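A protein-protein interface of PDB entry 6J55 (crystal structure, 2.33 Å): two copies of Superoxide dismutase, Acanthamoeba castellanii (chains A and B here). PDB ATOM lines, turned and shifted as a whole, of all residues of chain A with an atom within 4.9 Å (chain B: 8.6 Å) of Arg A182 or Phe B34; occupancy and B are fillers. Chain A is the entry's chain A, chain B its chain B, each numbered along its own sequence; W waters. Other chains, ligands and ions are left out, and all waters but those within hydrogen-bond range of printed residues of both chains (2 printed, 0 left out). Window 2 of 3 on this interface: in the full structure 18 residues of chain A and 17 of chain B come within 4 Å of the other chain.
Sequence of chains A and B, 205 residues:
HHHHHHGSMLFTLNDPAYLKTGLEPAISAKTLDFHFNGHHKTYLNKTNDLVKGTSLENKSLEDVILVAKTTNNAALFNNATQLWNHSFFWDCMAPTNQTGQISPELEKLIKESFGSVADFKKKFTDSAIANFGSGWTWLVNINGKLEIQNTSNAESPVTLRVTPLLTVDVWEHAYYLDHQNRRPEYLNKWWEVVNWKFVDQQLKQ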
ATOM      1  N   TYR A 176     -20.368   2.113  -5.273  1.00  0.00           N
ATOM      2  CA  TYR A 176     -20.140   3.372  -5.980  1.00  0.00           C
ATOM      3  C   TYR A 176     -18.995   3.265  -6.994  1.00  0.00           C
ATOM      4  O   TYR A 176     -19.033   3.937  -8.030  1.00  0.00           O
ATOM      5  CB  TYR A 176     -19.880   4.507  -4.986  1.00  0.00           C
ATOM      6  CG  TYR A 176     -20.437   5.822  -5.482  1.00  0.00           C
ATOM      7  CD1 TYR A 176     -21.790   6.090  -5.405  1.00  0.00           C
ATOM      8  CD2 TYR A 176     -19.616   6.771  -6.088  1.00  0.00           C
ATOM      9  CE1 TYR A 176     -22.305   7.273  -5.880  1.00  0.00           C
ATOM     10  CE2 TYR A 176     -20.130   7.965  -6.565  1.00  0.00           C
ATOM     11  CZ  TYR A 176     -21.475   8.207  -6.461  1.00  0.00           C
ATOM     12  OH  TYR A 176     -22.008   9.388  -6.924  1.00  0.00           O
ATOM     13  N   ASP A 178     -18.222   0.784  -8.915  1.00  0.00           N
ATOM     14  CA  ASP A 178     -18.712   0.106 -10.107  1.00  0.00           C
ATOM     15  C   ASP A 178     -19.955   0.752 -10.695  1.00  0.00           C
ATOM     16  O   ASP A 178     -20.146   0.710 -11.916  1.00  0.00           O
ATOM     17  CB  ASP A 178     -19.014  -1.361  -9.805  1.00  0.00           C
ATOM     18  CG  ASP A 178     -17.821  -2.083  -9.136  1.00  0.00           C
ATOM     19  OD1 ASP A 178     -16.671  -1.831  -9.549  1.00  0.00           O
ATOM     20  OD2 ASP A 178     -18.034  -2.943  -8.252  1.00  0.00           O
ATOM     21  N   HIS A 179     -20.821   1.341  -9.866  1.00  0.00           N
ATOM     22  CA  HIS A 179     -22.110   1.769 -10.366  1.00  0.00           C
ATOM     23  C   HIS A 179     -22.445   3.219 -10.103  1.00  0.00           C
ATOM     24  O   HIS A 179     -23.450   3.698 -10.646  1.00  0.00           O
ATOM     25  CB  HIS A 179     -23.220   0.883  -9.794  1.00  0.00           C
ATOM     26  CG  HIS A 179     -22.963  -0.572 -10.004  1.00  0.00           C
ATOM     27  ND1 HIS A 179     -23.188  -1.194 -11.215  1.00  0.00           N
ATOM     28  CD2 HIS A 179     -22.547  -1.538  -9.154  1.00  0.00           C
ATOM     29  CE1 HIS A 179     -22.878  -2.473 -11.111  1.00  0.00           C
ATOM     30  NE2 HIS A 179     -22.483  -2.709  -9.871  1.00  0.00           N
ATOM     31  N   GLN A 180     -21.605   3.939  -9.360  1.00  0.00           N
ATOM     32  CA  GLN A 180     -21.822   5.309  -8.926  1.00  0.00           C
ATOM     33  C   GLN A 180     -23.265   5.408  -8.425  1.00  0.00           C
ATOM     34  O   GLN A 180     -23.661   4.579  -7.594  1.00  0.00           O
ATOM     35  CB  GLN A 180     -21.445   6.273 -10.042  1.00  0.00           C
ATOM     36  CG  GLN A 180     -19.981   6.208 -10.526  1.00  0.00           C
ATOM     37  CD  GLN A 180     -19.752   5.096 -11.541  1.00  0.00           C
ATOM     38  OE1 GLN A 180     -20.473   4.995 -12.538  1.00  0.00           O
ATOM     39  NE2 GLN A 180     -18.735   4.284 -11.316  1.00  0.00           N
ATOM     40  N   ASN A 181     -24.065   6.372  -8.899  1.00  0.00           N
ATOM     41  CA  ASN A 181     -25.381   6.645  -8.332  1.00  0.00           C
ATOM     42  C   ASN A 181     -26.457   5.689  -8.821  1.00  0.00           C
ATOM     43  O   ASN A 181     -27.603   5.824  -8.398  1.00  0.00           O
ATOM     44  CB  ASN A 181     -25.775   8.095  -8.612  1.00  0.00           C
ATOM     45  CG  ASN A 181     -25.862   8.407 -10.092  1.00  0.00           C
ATOM     46  OD1 ASN A 181     -24.952   8.081 -10.886  1.00  0.00           O
ATOM     47  ND2 ASN A 181     -26.936   9.081 -10.476  1.00  0.00           N
ATOM     48  N   ARG A 182     -26.110   4.719  -9.666  1.00  0.00           N
ATOM     49  CA  ARG A 182     -27.073   3.779 -10.233  1.00  0.00           C
ATOM     50  C   ARG A 182     -27.232   2.550  -9.332  1.00  0.00           C
ATOM     51  O   ARG A 182     -26.921   1.422  -9.707  1.00  0.00           O
ATOM     52  CB  ARG A 182     -26.631   3.373 -11.637  1.00  0.00           C
ATOM     53  CG  ARG A 182     -26.213   4.556 -12.531  1.00  0.00           C
ATOM     54  CD  ARG A 182     -25.739   4.084 -13.899  1.00  0.00           C
ATOM     55  NE  ARG A 182     -24.479   3.325 -13.844  1.00  0.00           N
ATOM     56  CZ  ARG A 182     -23.273   3.858 -13.677  1.00  0.00           C
ATOM     57  NH1 ARG A 182     -23.123   5.163 -13.522  1.00  0.00           N
ATOM     58  NH2 ARG A 182     -22.211   3.076 -13.658  1.00  0.00           N
ATOM     59  N   ARG A 183     -27.728   2.779  -8.118  1.00  0.00           N
ATOM     60  CA  ARG A 183     -28.031   1.653  -7.239  1.00  0.00           C
ATOM     61  C   ARG A 183     -28.955   0.633  -7.877  1.00  0.00           C
ATOM     62  O   ARG A 183     -28.711  -0.574  -7.682  1.00  0.00           O
ATOM     63  CB  ARG A 183     -28.654   2.146  -5.926  1.00  0.00           C
ATOM     64  CG  ARG A 183     -28.750   1.058  -4.829  1.00  0.00           C
ATOM     65  CD  ARG A 183     -29.648   1.499  -3.695  1.00  0.00           C
ATOM     66  NE  ARG A 183     -28.943   2.433  -2.845  1.00  0.00           N
ATOM     67  CZ  ARG A 183     -29.439   2.915  -1.713  1.00  0.00           C
ATOM     68  NH1 ARG A 183     -30.648   2.540  -1.313  1.00  0.00           N
ATOM     69  NH2 ARG A 183     -28.734   3.760  -0.977  1.00  0.00           N
ATOM     70  N   PRO A 184     -30.002   1.006  -8.634  1.00  0.00           N
ATOM     71  CA  PRO A 184     -30.831  -0.032  -9.270  1.00  0.00           C
ATOM     72  C   PRO A 184     -30.037  -0.973 -10.160  1.00  0.00           C
ATOM     73  O   PRO A 184     -30.294  -2.182 -10.162  1.00  0.00           O
ATOM     74  CB  PRO A 184     -31.874   0.778 -10.072  1.00  0.00           C
ATOM     75  CG  PRO A 184     -31.939   2.097  -9.382  1.00  0.00           C
ATOM     76  CD  PRO A 184     -30.573   2.359  -8.814  1.00  0.00           C
ATOM     77  N   GLU A 185     -29.075  -0.443 -10.917  1.00  0.00           N
ATOM     78  CA  GLU A 185     -28.233  -1.286 -11.757  1.00  0.00           C
ATOM     79  C   GLU A 185     -27.380  -2.209 -10.890  1.00  0.00           C
ATOM     80  O   GLU A 185     -27.239  -3.397 -11.193  1.00  0.00           O
ATOM     81  CB  GLU A 185     -27.354  -0.381 -12.634  1.00  0.00           C
ATOM     82  CG  GLU A 185     -26.094  -1.024 -13.256  1.00  0.00           C
ATOM     83  CD  GLU A 185     -25.179  -0.004 -13.974  1.00  0.00           C
ATOM     84  OE1 GLU A 185     -25.730   0.897 -14.648  1.00  0.00           O
ATOM     85  OE2 GLU A 185     -23.915  -0.061 -13.801  1.00  0.00           O
ATOM     86  N   TYR A 186     -26.917  -1.713  -9.738  1.00  0.00           N
ATOM     87  CA  TYR A 186     -26.190  -2.560  -8.792  1.00  0.00           C
ATOM     88  C   TYR A 186     -27.061  -3.698  -8.278  1.00  0.00           C
ATOM     89  O   TYR A 186     -26.658  -4.860  -8.315  1.00  0.00           O
ATOM     90  CB  TYR A 186     -25.677  -1.712  -7.630  1.00  0.00           C
ATOM     91  CG  TYR A 186     -25.358  -2.452  -6.321  1.00  0.00           C
ATOM     92  CD1 TYR A 186     -26.004  -2.121  -5.134  1.00  0.00           C
ATOM     93  CD2 TYR A 186     -24.346  -3.415  -6.262  1.00  0.00           C
ATOM     94  CE1 TYR A 186     -25.673  -2.764  -3.926  1.00  0.00           C
ATOM     95  CE2 TYR A 186     -24.019  -4.056  -5.070  1.00  0.00           C
ATOM     96  CZ  TYR A 186     -24.668  -3.721  -3.910  1.00  0.00           C
ATOM     97  OH  TYR A 186     -24.338  -4.370  -2.737  1.00  0.00           O
ATOM     98  N   LEU B  19     -17.401  23.348 -11.927  1.00  0.00           N
ATOM     99  CA  LEU B  19     -17.939  22.020 -12.219  1.00  0.00           C
ATOM    100  C   LEU B  19     -16.999  21.207 -13.093  1.00  0.00           C
ATOM    101  O   LEU B  19     -16.793  20.007 -12.856  1.00  0.00           O
ATOM    102  CB  LEU B  19     -19.299  22.143 -12.905  1.00  0.00           C
ATOM    103  CG  LEU B  19     -19.935  20.845 -13.391  1.00  0.00           C
ATOM    104  CD1 LEU B  19     -20.043  19.853 -12.267  1.00  0.00           C
ATOM    105  CD2 LEU B  19     -21.298  21.123 -14.001  1.00  0.00           C
ATOM    106  N   SER B  28     -12.476  15.641  -7.249  1.00  0.00           N
ATOM    107  CA  SER B  28     -12.157  15.625  -8.672  1.00  0.00           C
ATOM    108  C   SER B  28     -13.347  16.068  -9.523  1.00  0.00           C
ATOM    109  O   SER B  28     -14.509  15.963  -9.124  1.00  0.00           O
ATOM    110  CB  SER B  28     -11.725  14.239  -9.127  1.00  0.00           C
ATOM    111  OG  SER B  28     -12.823  13.353  -9.232  1.00  0.00           O
ATOM    112  N   ALA B  29     -13.044  16.480 -10.756  1.00  0.00           N
ATOM    113  CA  ALA B  29     -14.098  16.878 -11.678  1.00  0.00           C
ATOM    114  C   ALA B  29     -15.037  15.727 -11.952  1.00  0.00           C
ATOM    115  O   ALA B  29     -16.241  15.928 -12.128  1.00  0.00           O
ATOM    116  CB  ALA B  29     -13.502  17.389 -12.991  1.00  0.00           C
ATOM    117  N   LYS B  30     -14.504  14.508 -11.980  1.00  0.00           N
ATOM    118  CA  LYS B  30     -15.347  13.342 -12.201  1.00  0.00           C
ATOM    119  C   LYS B  30     -16.336  13.148 -11.055  1.00  0.00           C
ATOM    120  O   LYS B  30     -17.479  12.753 -11.276  1.00  0.00           O
ATOM    121  CB  LYS B  30     -14.475  12.099 -12.368  1.00  0.00           C
ATOM    122  CG  LYS B  30     -15.251  10.949 -12.949  1.00  0.00           C
ATOM    123  CD  LYS B  30     -14.882   9.617 -12.327  1.00  0.00           C
ATOM    124  CE  LYS B  30     -13.642   9.043 -12.959  1.00  0.00           C
ATOM    125  NZ  LYS B  30     -13.647   7.559 -12.812  1.00  0.00           N
ATOM    126  N   THR B  31     -15.911  13.411  -9.820  1.00  0.00           N
ATOM    127  CA  THR B  31     -16.843  13.297  -8.704  1.00  0.00           C
ATOM    128  C   THR B  31     -17.934  14.357  -8.794  1.00  0.00           C
ATOM    129  O   THR B  31     -19.111  14.065  -8.554  1.00  0.00           O
ATOM    130  CB  THR B  31     -16.103  13.407  -7.369  1.00  0.00           C
ATOM    131  OG1 THR B  31     -15.536  12.132  -7.052  1.00  0.00           O
ATOM    132  CG2 THR B  31     -17.080  13.798  -6.246  1.00  0.00           C
ATOM    133  N   LEU B  32     -17.571  15.576  -9.194  1.00  0.00           N
ATOM    134  CA  LEU B  32     -18.570  16.627  -9.271  1.00  0.00           C
ATOM    135  C   LEU B  32     -19.590  16.311 -10.344  1.00  0.00           C
ATOM    136  O   LEU B  32     -20.769  16.618 -10.175  1.00  0.00           O
ATOM    137  CB  LEU B  32     -17.894  17.968  -9.551  1.00  0.00           C
ATOM    138  CG  LEU B  32     -17.144  18.520  -8.343  1.00  0.00           C
ATOM    139  CD1 LEU B  32     -16.286  19.721  -8.747  1.00  0.00           C
ATOM    140  CD2 LEU B  32     -18.100  18.877  -7.229  1.00  0.00           C
ATOM    141  N   ASP B  33     -19.186  15.568 -11.369  1.00  0.00           N
ATOM    142  CA  ASP B  33     -20.117  15.184 -12.422  1.00  0.00           C
ATOM    143  C   ASP B  33     -21.208  14.266 -11.877  1.00  0.00           C
ATOM    144  O   ASP B  33     -22.405  14.540 -12.042  1.00  0.00           O
ATOM    145  CB  ASP B  33     -19.346  14.507 -13.561  1.00  0.00           C
ATOM    146  CG  ASP B  33     -20.231  14.155 -14.754  1.00  0.00           C
ATOM    147  OD1 ASP B  33     -21.254  14.831 -15.005  1.00  0.00           O
ATOM    148  OD2 ASP B  33     -19.897  13.182 -15.451  1.00  0.00           O
ATOM    149  N   PHE B  34     -20.816  13.178 -11.199  1.00  0.00           N
ATOM    150  CA  PHE B  34     -21.812  12.298 -10.599  1.00  0.00           C
ATOM    151  C   PHE B  34     -22.521  12.991  -9.438  1.00  0.00           C
ATOM    152  O   PHE B  34     -23.713  12.778  -9.212  1.00  0.00           O
ATOM    153  CB  PHE B  34     -21.154  10.991 -10.121  1.00  0.00           C
ATOM    154  CG  PHE B  34     -20.665  10.098 -11.237  1.00  0.00           C
ATOM    155  CD1 PHE B  34     -21.555   9.337 -11.967  1.00  0.00           C
ATOM    156  CD2 PHE B  34     -19.316  10.020 -11.549  1.00  0.00           C
ATOM    157  CE1 PHE B  34     -21.126   8.516 -12.987  1.00  0.00           C
ATOM    158  CE2 PHE B  34     -18.880   9.186 -12.581  1.00  0.00           C
ATOM    159  CZ  PHE B  34     -19.799   8.440 -13.291  1.00  0.00           C
ATOM    160  N   HIS B  35     -21.803  13.805  -8.675  1.00  0.00           N
ATOM    161  CA  HIS B  35     -22.404  14.428  -7.500  1.00  0.00           C
ATOM    162  C   HIS B  35     -23.471  15.453  -7.901  1.00  0.00           C
ATOM    163  O   HIS B  35     -24.594  15.442  -7.381  1.00  0.00           O
ATOM    164  CB  HIS B  35     -21.303  15.088  -6.672  1.00  0.00           C
ATOM    165  CG  HIS B  35     -21.622  15.250  -5.220  1.00  0.00           C
ATOM    166  ND1 HIS B  35     -20.662  15.595  -4.284  1.00  0.00           N
ATOM    167  CD2 HIS B  35     -22.785  15.122  -4.539  1.00  0.00           C
ATOM    168  CE1 HIS B  35     -21.230  15.701  -3.098  1.00  0.00           C
ATOM    169  NE2 HIS B  35     -22.513  15.411  -3.224  1.00  0.00           N
ATOM    170  N   PHE B  36     -23.151  16.310  -8.867  1.00  0.00           N
ATOM    171  CA  PHE B  36     -24.071  17.356  -9.278  1.00  0.00           C
ATOM    172  C   PHE B  36     -25.035  16.852 -10.345  1.00  0.00           C
ATOM    173  O   PHE B  36     -26.253  16.910 -10.156  1.00  0.00           O
ATOM    174  CB  PHE B  36     -23.280  18.573  -9.775  1.00  0.00           C
ATOM    175  CG  PHE B  36     -24.149  19.680 -10.315  1.00  0.00           C
ATOM    176  CD1 PHE B  36     -24.855  20.505  -9.449  1.00  0.00           C
ATOM    177  CD2 PHE B  36     -24.268  19.887 -11.688  1.00  0.00           C
ATOM    178  CE1 PHE B  36     -25.660  21.529  -9.942  1.00  0.00           C
ATOM    179  CE2 PHE B  36     -25.069  20.912 -12.195  1.00  0.00           C
ATOM    180  CZ  PHE B  36     -25.764  21.738 -11.326  1.00  0.00           C
ATOM    181  N   ASN B  37     -24.511  16.332 -11.458  1.00  0.00           N
ATOM    182  CA  ASN B  37     -25.390  15.874 -12.531  1.00  0.00           C
ATOM    183  C   ASN B  37     -26.112  14.597 -12.154  1.00  0.00           C
ATOM    184  O   ASN B  37     -27.195  14.322 -12.680  1.00  0.00           O
ATOM    185  CB  ASN B  37     -24.590  15.676 -13.823  1.00  0.00           C
ATOM    186  CG  ASN B  37     -24.097  16.989 -14.397  1.00  0.00           C
ATOM    187  OD1 ASN B  37     -24.887  17.891 -14.628  1.00  0.00           O
ATOM    188  ND2 ASN B  37     -22.791  17.127 -14.552  1.00  0.00           N
ATOM    189  N   GLY B  38     -25.528  13.796 -11.260  1.00  0.00           N
ATOM    190  CA  GLY B  38     -26.197  12.606 -10.779  1.00  0.00           C
ATOM    191  C   GLY B  38     -27.068  12.900  -9.576  1.00  0.00           C
ATOM    192  O   GLY B  38     -28.296  12.959  -9.708  1.00  0.00           O
ATOM    193  N   HIS B  39     -26.450  13.056  -8.392  1.00  0.00           N
ATOM    194  CA  HIS B  39     -27.216  13.160  -7.151  1.00  0.00           C
ATOM    195  C   HIS B  39     -28.040  14.460  -7.083  1.00  0.00           C
ATOM    196  O   HIS B  39     -29.239  14.425  -6.783  1.00  0.00           O
ATOM    197  CB  HIS B  39     -26.283  13.006  -5.937  1.00  0.00           C
ATOM    198  CG  HIS B  39     -25.608  11.664  -5.861  1.00  0.00           C
ATOM    199  ND1 HIS B  39     -26.254  10.530  -5.420  1.00  0.00           N
ATOM    200  CD2 HIS B  39     -24.359  11.268  -6.203  1.00  0.00           C
ATOM    201  CE1 HIS B  39     -25.432   9.498  -5.485  1.00  0.00           C
ATOM    202  NE2 HIS B  39     -24.275   9.922  -5.947  1.00  0.00           N
ATOM    203  N   HIS B  40     -27.414  15.623  -7.308  1.00  0.00           N
ATOM    204  CA  HIS B  40     -28.129  16.882  -7.064  1.00  0.00           C
ATOM    205  C   HIS B  40     -29.320  17.044  -8.008  1.00  0.00           C
ATOM    206  O   HIS B  40     -30.417  17.420  -7.572  1.00  0.00           O
ATOM    207  CB  HIS B  40     -27.175  18.074  -7.176  1.00  0.00           C
ATOM    208  CG  HIS B  40     -27.641  19.303  -6.442  1.00  0.00           C
ATOM    209  ND1 HIS B  40     -26.894  20.462  -6.370  1.00  0.00           N
ATOM    210  CD2 HIS B  40     -28.772  19.551  -5.734  1.00  0.00           C
ATOM    211  CE1 HIS B  40     -27.535  21.361  -5.645  1.00  0.00           C
ATOM    212  NE2 HIS B  40     -28.680  20.837  -5.248  1.00  0.00           N
ATOM    213  N   LYS B  41     -29.147  16.707  -9.286  1.00  0.00           N
ATOM    214  CA  LYS B  41     -30.251  16.832 -10.236  1.00  0.00           C
ATOM    215  C   LYS B  41     -31.341  15.810  -9.992  1.00  0.00           C
ATOM    216  O   LYS B  41     -32.515  16.076 -10.299  1.00  0.00           O
ATOM    217  CB  LYS B  41     -29.758  16.704 -11.680  1.00  0.00           C
ATOM    218  CG  LYS B  41     -29.191  17.995 -12.206  1.00  0.00           C
ATOM    219  CD  LYS B  41     -28.619  17.862 -13.600  1.00  0.00           C
ATOM    220  CE  LYS B  41     -28.043  19.219 -14.034  1.00  0.00           C
ATOM    221  NZ  LYS B  41     -27.530  19.201 -15.438  1.00  0.00           N
ATOM    222  N   THR B  42     -30.982  14.627  -9.491  1.00  0.00           N
ATOM    223  CA  THR B  42     -32.015  13.668  -9.107  1.00  0.00           C
ATOM    224  C   THR B  42     -32.879  14.224  -7.976  1.00  0.00           C
ATOM    225  O   THR B  42     -34.111  14.102  -8.011  1.00  0.00           O
ATOM    226  CB  THR B  42     -31.383  12.329  -8.722  1.00  0.00           C
ATOM    227  OG1 THR B  42     -30.713  11.791  -9.864  1.00  0.00           O
ATOM    228  CG2 THR B  42     -32.441  11.333  -8.297  1.00  0.00           C
ATOM    229  N   TYR B  43     -32.254  14.830  -6.962  1.00  0.00           N
ATOM    230  CA  TYR B  43     -33.021  15.450  -5.874  1.00  0.00           C
ATOM    231  C   TYR B  43     -33.911  16.584  -6.385  1.00  0.00           C
ATOM    232  O   TYR B  43     -35.021  16.782  -5.883  1.00  0.00           O
ATOM    233  CB  TYR B  43     -32.089  15.969  -4.774  1.00  0.00           C
ATOM    234  CG  TYR B  43     -31.357  14.896  -4.008  1.00  0.00           C
ATOM    235  CD1 TYR B  43     -29.988  15.016  -3.738  1.00  0.00           C
ATOM    236  CD2 TYR B  43     -32.033  13.789  -3.505  1.00  0.00           C
ATOM    237  CE1 TYR B  43     -29.299  14.033  -3.009  1.00  0.00           C
ATOM    238  CE2 TYR B  43     -31.364  12.792  -2.780  1.00  0.00           C
ATOM    239  CZ  TYR B  43     -30.000  12.913  -2.532  1.00  0.00           C
ATOM    240  OH  TYR B  43     -29.346  11.931  -1.815  1.00  0.00           O
ATOM    241  N   HIS B  86     -27.109  20.438  -0.926  1.00  0.00           N
ATOM    242  CA  HIS B  86     -26.042  20.489  -1.906  1.00  0.00           C
ATOM    243  C   HIS B  86     -25.836  21.903  -2.429  1.00  0.00           C
ATOM    244  O   HIS B  86     -24.685  22.337  -2.585  1.00  0.00           O
ATOM    245  CB  HIS B  86     -26.333  19.529  -3.046  1.00  0.00           C
ATOM    246  CG  HIS B  86     -26.278  18.103  -2.629  1.00  0.00           C
ATOM    247  ND1 HIS B  86     -27.355  17.458  -2.064  1.00  0.00           N
ATOM    248  CD2 HIS B  86     -25.265  17.207  -2.639  1.00  0.00           C
ATOM    249  CE1 HIS B  86     -27.021  16.219  -1.768  1.00  0.00           C
ATOM    250  NE2 HIS B  86     -25.766  16.037  -2.125  1.00  0.00           N
ATOM    251  N   TRP B  90     -22.141  23.634  -2.436  1.00  0.00           N
ATOM    252  CA  TRP B  90     -21.359  24.168  -3.550  1.00  0.00           C
ATOM    253  C   TRP B  90     -20.864  25.577  -3.250  1.00  0.00           C
ATOM    254  O   TRP B  90     -19.740  25.933  -3.624  1.00  0.00           O
ATOM    255  CB  TRP B  90     -22.160  24.174  -4.844  1.00  0.00           C
ATOM    256  CG  TRP B  90     -22.745  22.869  -5.258  1.00  0.00           C
ATOM    257  CD1 TRP B  90     -23.987  22.686  -5.767  1.00  0.00           C
ATOM    258  CD2 TRP B  90     -22.133  21.563  -5.209  1.00  0.00           C
ATOM    259  NE1 TRP B  90     -24.191  21.360  -6.058  1.00  0.00           N
ATOM    260  CE2 TRP B  90     -23.077  20.647  -5.710  1.00  0.00           C
ATOM    261  CE3 TRP B  90     -20.888  21.081  -4.788  1.00  0.00           C
ATOM    262  CZ2 TRP B  90     -22.817  19.283  -5.806  1.00  0.00           C
ATOM    263  CZ3 TRP B  90     -20.630  19.731  -4.892  1.00  0.00           C
ATOM    264  CH2 TRP B  90     -21.581  18.845  -5.402  1.00  0.00           C
ATOM    265  N   HIS B 173     -20.848   9.054  -1.395  1.00  0.00           N
ATOM    266  CA  HIS B 173     -20.728   9.481  -2.781  1.00  0.00           C
ATOM    267  C   HIS B 173     -19.987  10.804  -2.909  1.00  0.00           C
ATOM    268  O   HIS B 173     -19.528  11.126  -4.004  1.00  0.00           O
ATOM    269  CB  HIS B 173     -22.096   9.559  -3.501  1.00  0.00           C
ATOM    270  CG  HIS B 173     -23.056  10.547  -2.925  1.00  0.00           C
ATOM    271  ND1 HIS B 173     -24.323  10.187  -2.520  1.00  0.00           N
ATOM    272  CD2 HIS B 173     -22.934  11.870  -2.657  1.00  0.00           C
ATOM    273  CE1 HIS B 173     -24.943  11.250  -2.035  1.00  0.00           C
ATOM    274  NE2 HIS B 173     -24.123  12.285  -2.109  1.00  0.00           N
ATOM    275  N   ALA B 174     -19.847  11.575  -1.830  1.00  0.00           N
ATOM    276  CA  ALA B 174     -19.119  12.837  -1.933  1.00  0.00           C
ATOM    277  C   ALA B 174     -17.624  12.641  -2.147  1.00  0.00           C
ATOM    278  O   ALA B 174     -16.954  13.569  -2.631  1.00  0.00           O
ATOM    279  CB  ALA B 174     -19.299  13.682  -0.680  1.00  0.00           C
ATOM    280  N   LEU B 177     -15.069   8.073  -4.964  1.00  0.00           N
ATOM    281  CA  LEU B 177     -14.318   7.924  -6.210  1.00  0.00           C
ATOM    282  C   LEU B 177     -12.902   8.469  -6.079  1.00  0.00           C
ATOM    283  O   LEU B 177     -11.980   7.945  -6.710  1.00  0.00           O
ATOM    284  CB  LEU B 177     -15.035   8.608  -7.366  1.00  0.00           C
ATOM    285  CG  LEU B 177     -16.383   8.037  -7.806  1.00  0.00           C
ATOM    286  CD1 LEU B 177     -17.007   8.970  -8.831  1.00  0.00           C
ATOM    287  CD2 LEU B 177     -16.197   6.659  -8.403  1.00  0.00           C
HETATM  288  O   HOH W   1     -20.856  11.645  -6.600  1.00  0.00           O
HETATM  289  O   HOH W   2     -29.040   9.824  -9.040  1.00  0.00           O
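Of the 22 printed residues of chain B, 5 touch a printed residue of chain A. Printed residues of chain B that touch a printed residue of chain A: Phe B34, Gly B38, His B39, His B173 and Leu B177. Of the 10 printed residues of chain A, 4 touch a printed residue of chain B. Among the printed residues, 9 pairs touch across the chains.
Phe B34 touches Tyr A176 (CB to OH, 3.7 Å). His B173 touches Tyr A176 (CB to CE1, 3.3 Å). CD2 of Tyr A176 touches CG of Leu B177, at 3.9 Å. Phe B34 touches Gln A180. CD1 of Phe B34 touches OD1 of Asn A181, 3.8 Å away. Asn A181 touches Gly B38 (ND2 to CA, 3.6 Å). CB of Asn A181 touches CE1 of His B39, 3.4 Å away. Arg A182 touches Phe B34 (NH1 to CE1, 3.9 Å).
Water W1 lies within hydrogen-bond range of OH of Tyr A176, O of His B173 and N of His B35. Water W2 lies within hydrogen-bond range of the side-chain amide nitrogen (ND2) of Asn A181 (2.7 Å), the side-chain hydroxyl (OG1) of Thr B42 (2.7 Å) and the backbone carbonyl oxygen (O) of Gly B38 (3.3 Å).
O of Gly B38 sits at hydrogen-bond distance from OG1 of Thr B42. The side-chain amide oxygen of Gln A180 sits at hydrogen-bond distance from the guanidinium group of Arg A182. A ring nitrogen (NE2) of His B39 lies close to a ring nitrogen (ND1) of His B173 (3.4 Å). NE2 of Gln A180 sits close to O of Tyr A176, 3.3 Å away. O of Asp B33 sits at hydrogen-bond distance from N of Gly B38 (3.3 Å). NH1 of Arg A182 sits close to O of His A179 (3.2 Å).
No position is printed for both chains. Of the 9 pairs that touch across the chains among the printed residues, none has its exchanged pair printed and touching as well.
The side-chain hydroxyl (OH) of Tyr A176 is in hydrogen-bond range of a ring nitrogen (NE2) of His B39 (2.5 Å).
Of the printed residues of chain B, Tyr A176 touches Phe B34 (3.7 Å), His B39 (2.5 Å), His B173 (3.3 Å) and Leu B177 (3.9 Å). Asn A181 touches just these residues of chain B: Phe B34 (3.8 Å), Gly B38 (3.6 Å) and His B39 (3.4 Å). Arg A182 touches one residue of chain B. Of chain A, only Tyr A176, Gln A180, Asn A181 and Arg A182 come within 4 Å of Phe B34. Printed residues of chain A within 4 Å of Gly B38: Asn A181 (3.6 Å). Printed residues of chain A within 4 Å of His B39: Tyr A176 and Asn A181. Of the printed residues of chain A, His B173 touches Tyr A176. Printed residues of chain A within 4 Å of Leu B177: Tyr A176 (3.9 Å). The nearest residue of chain B that does not touch Arg A182 is His B39 (6.4 Å). The nearest printed residue of chain A that does not touch His B39 is Gln A180 (5.2 Å).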
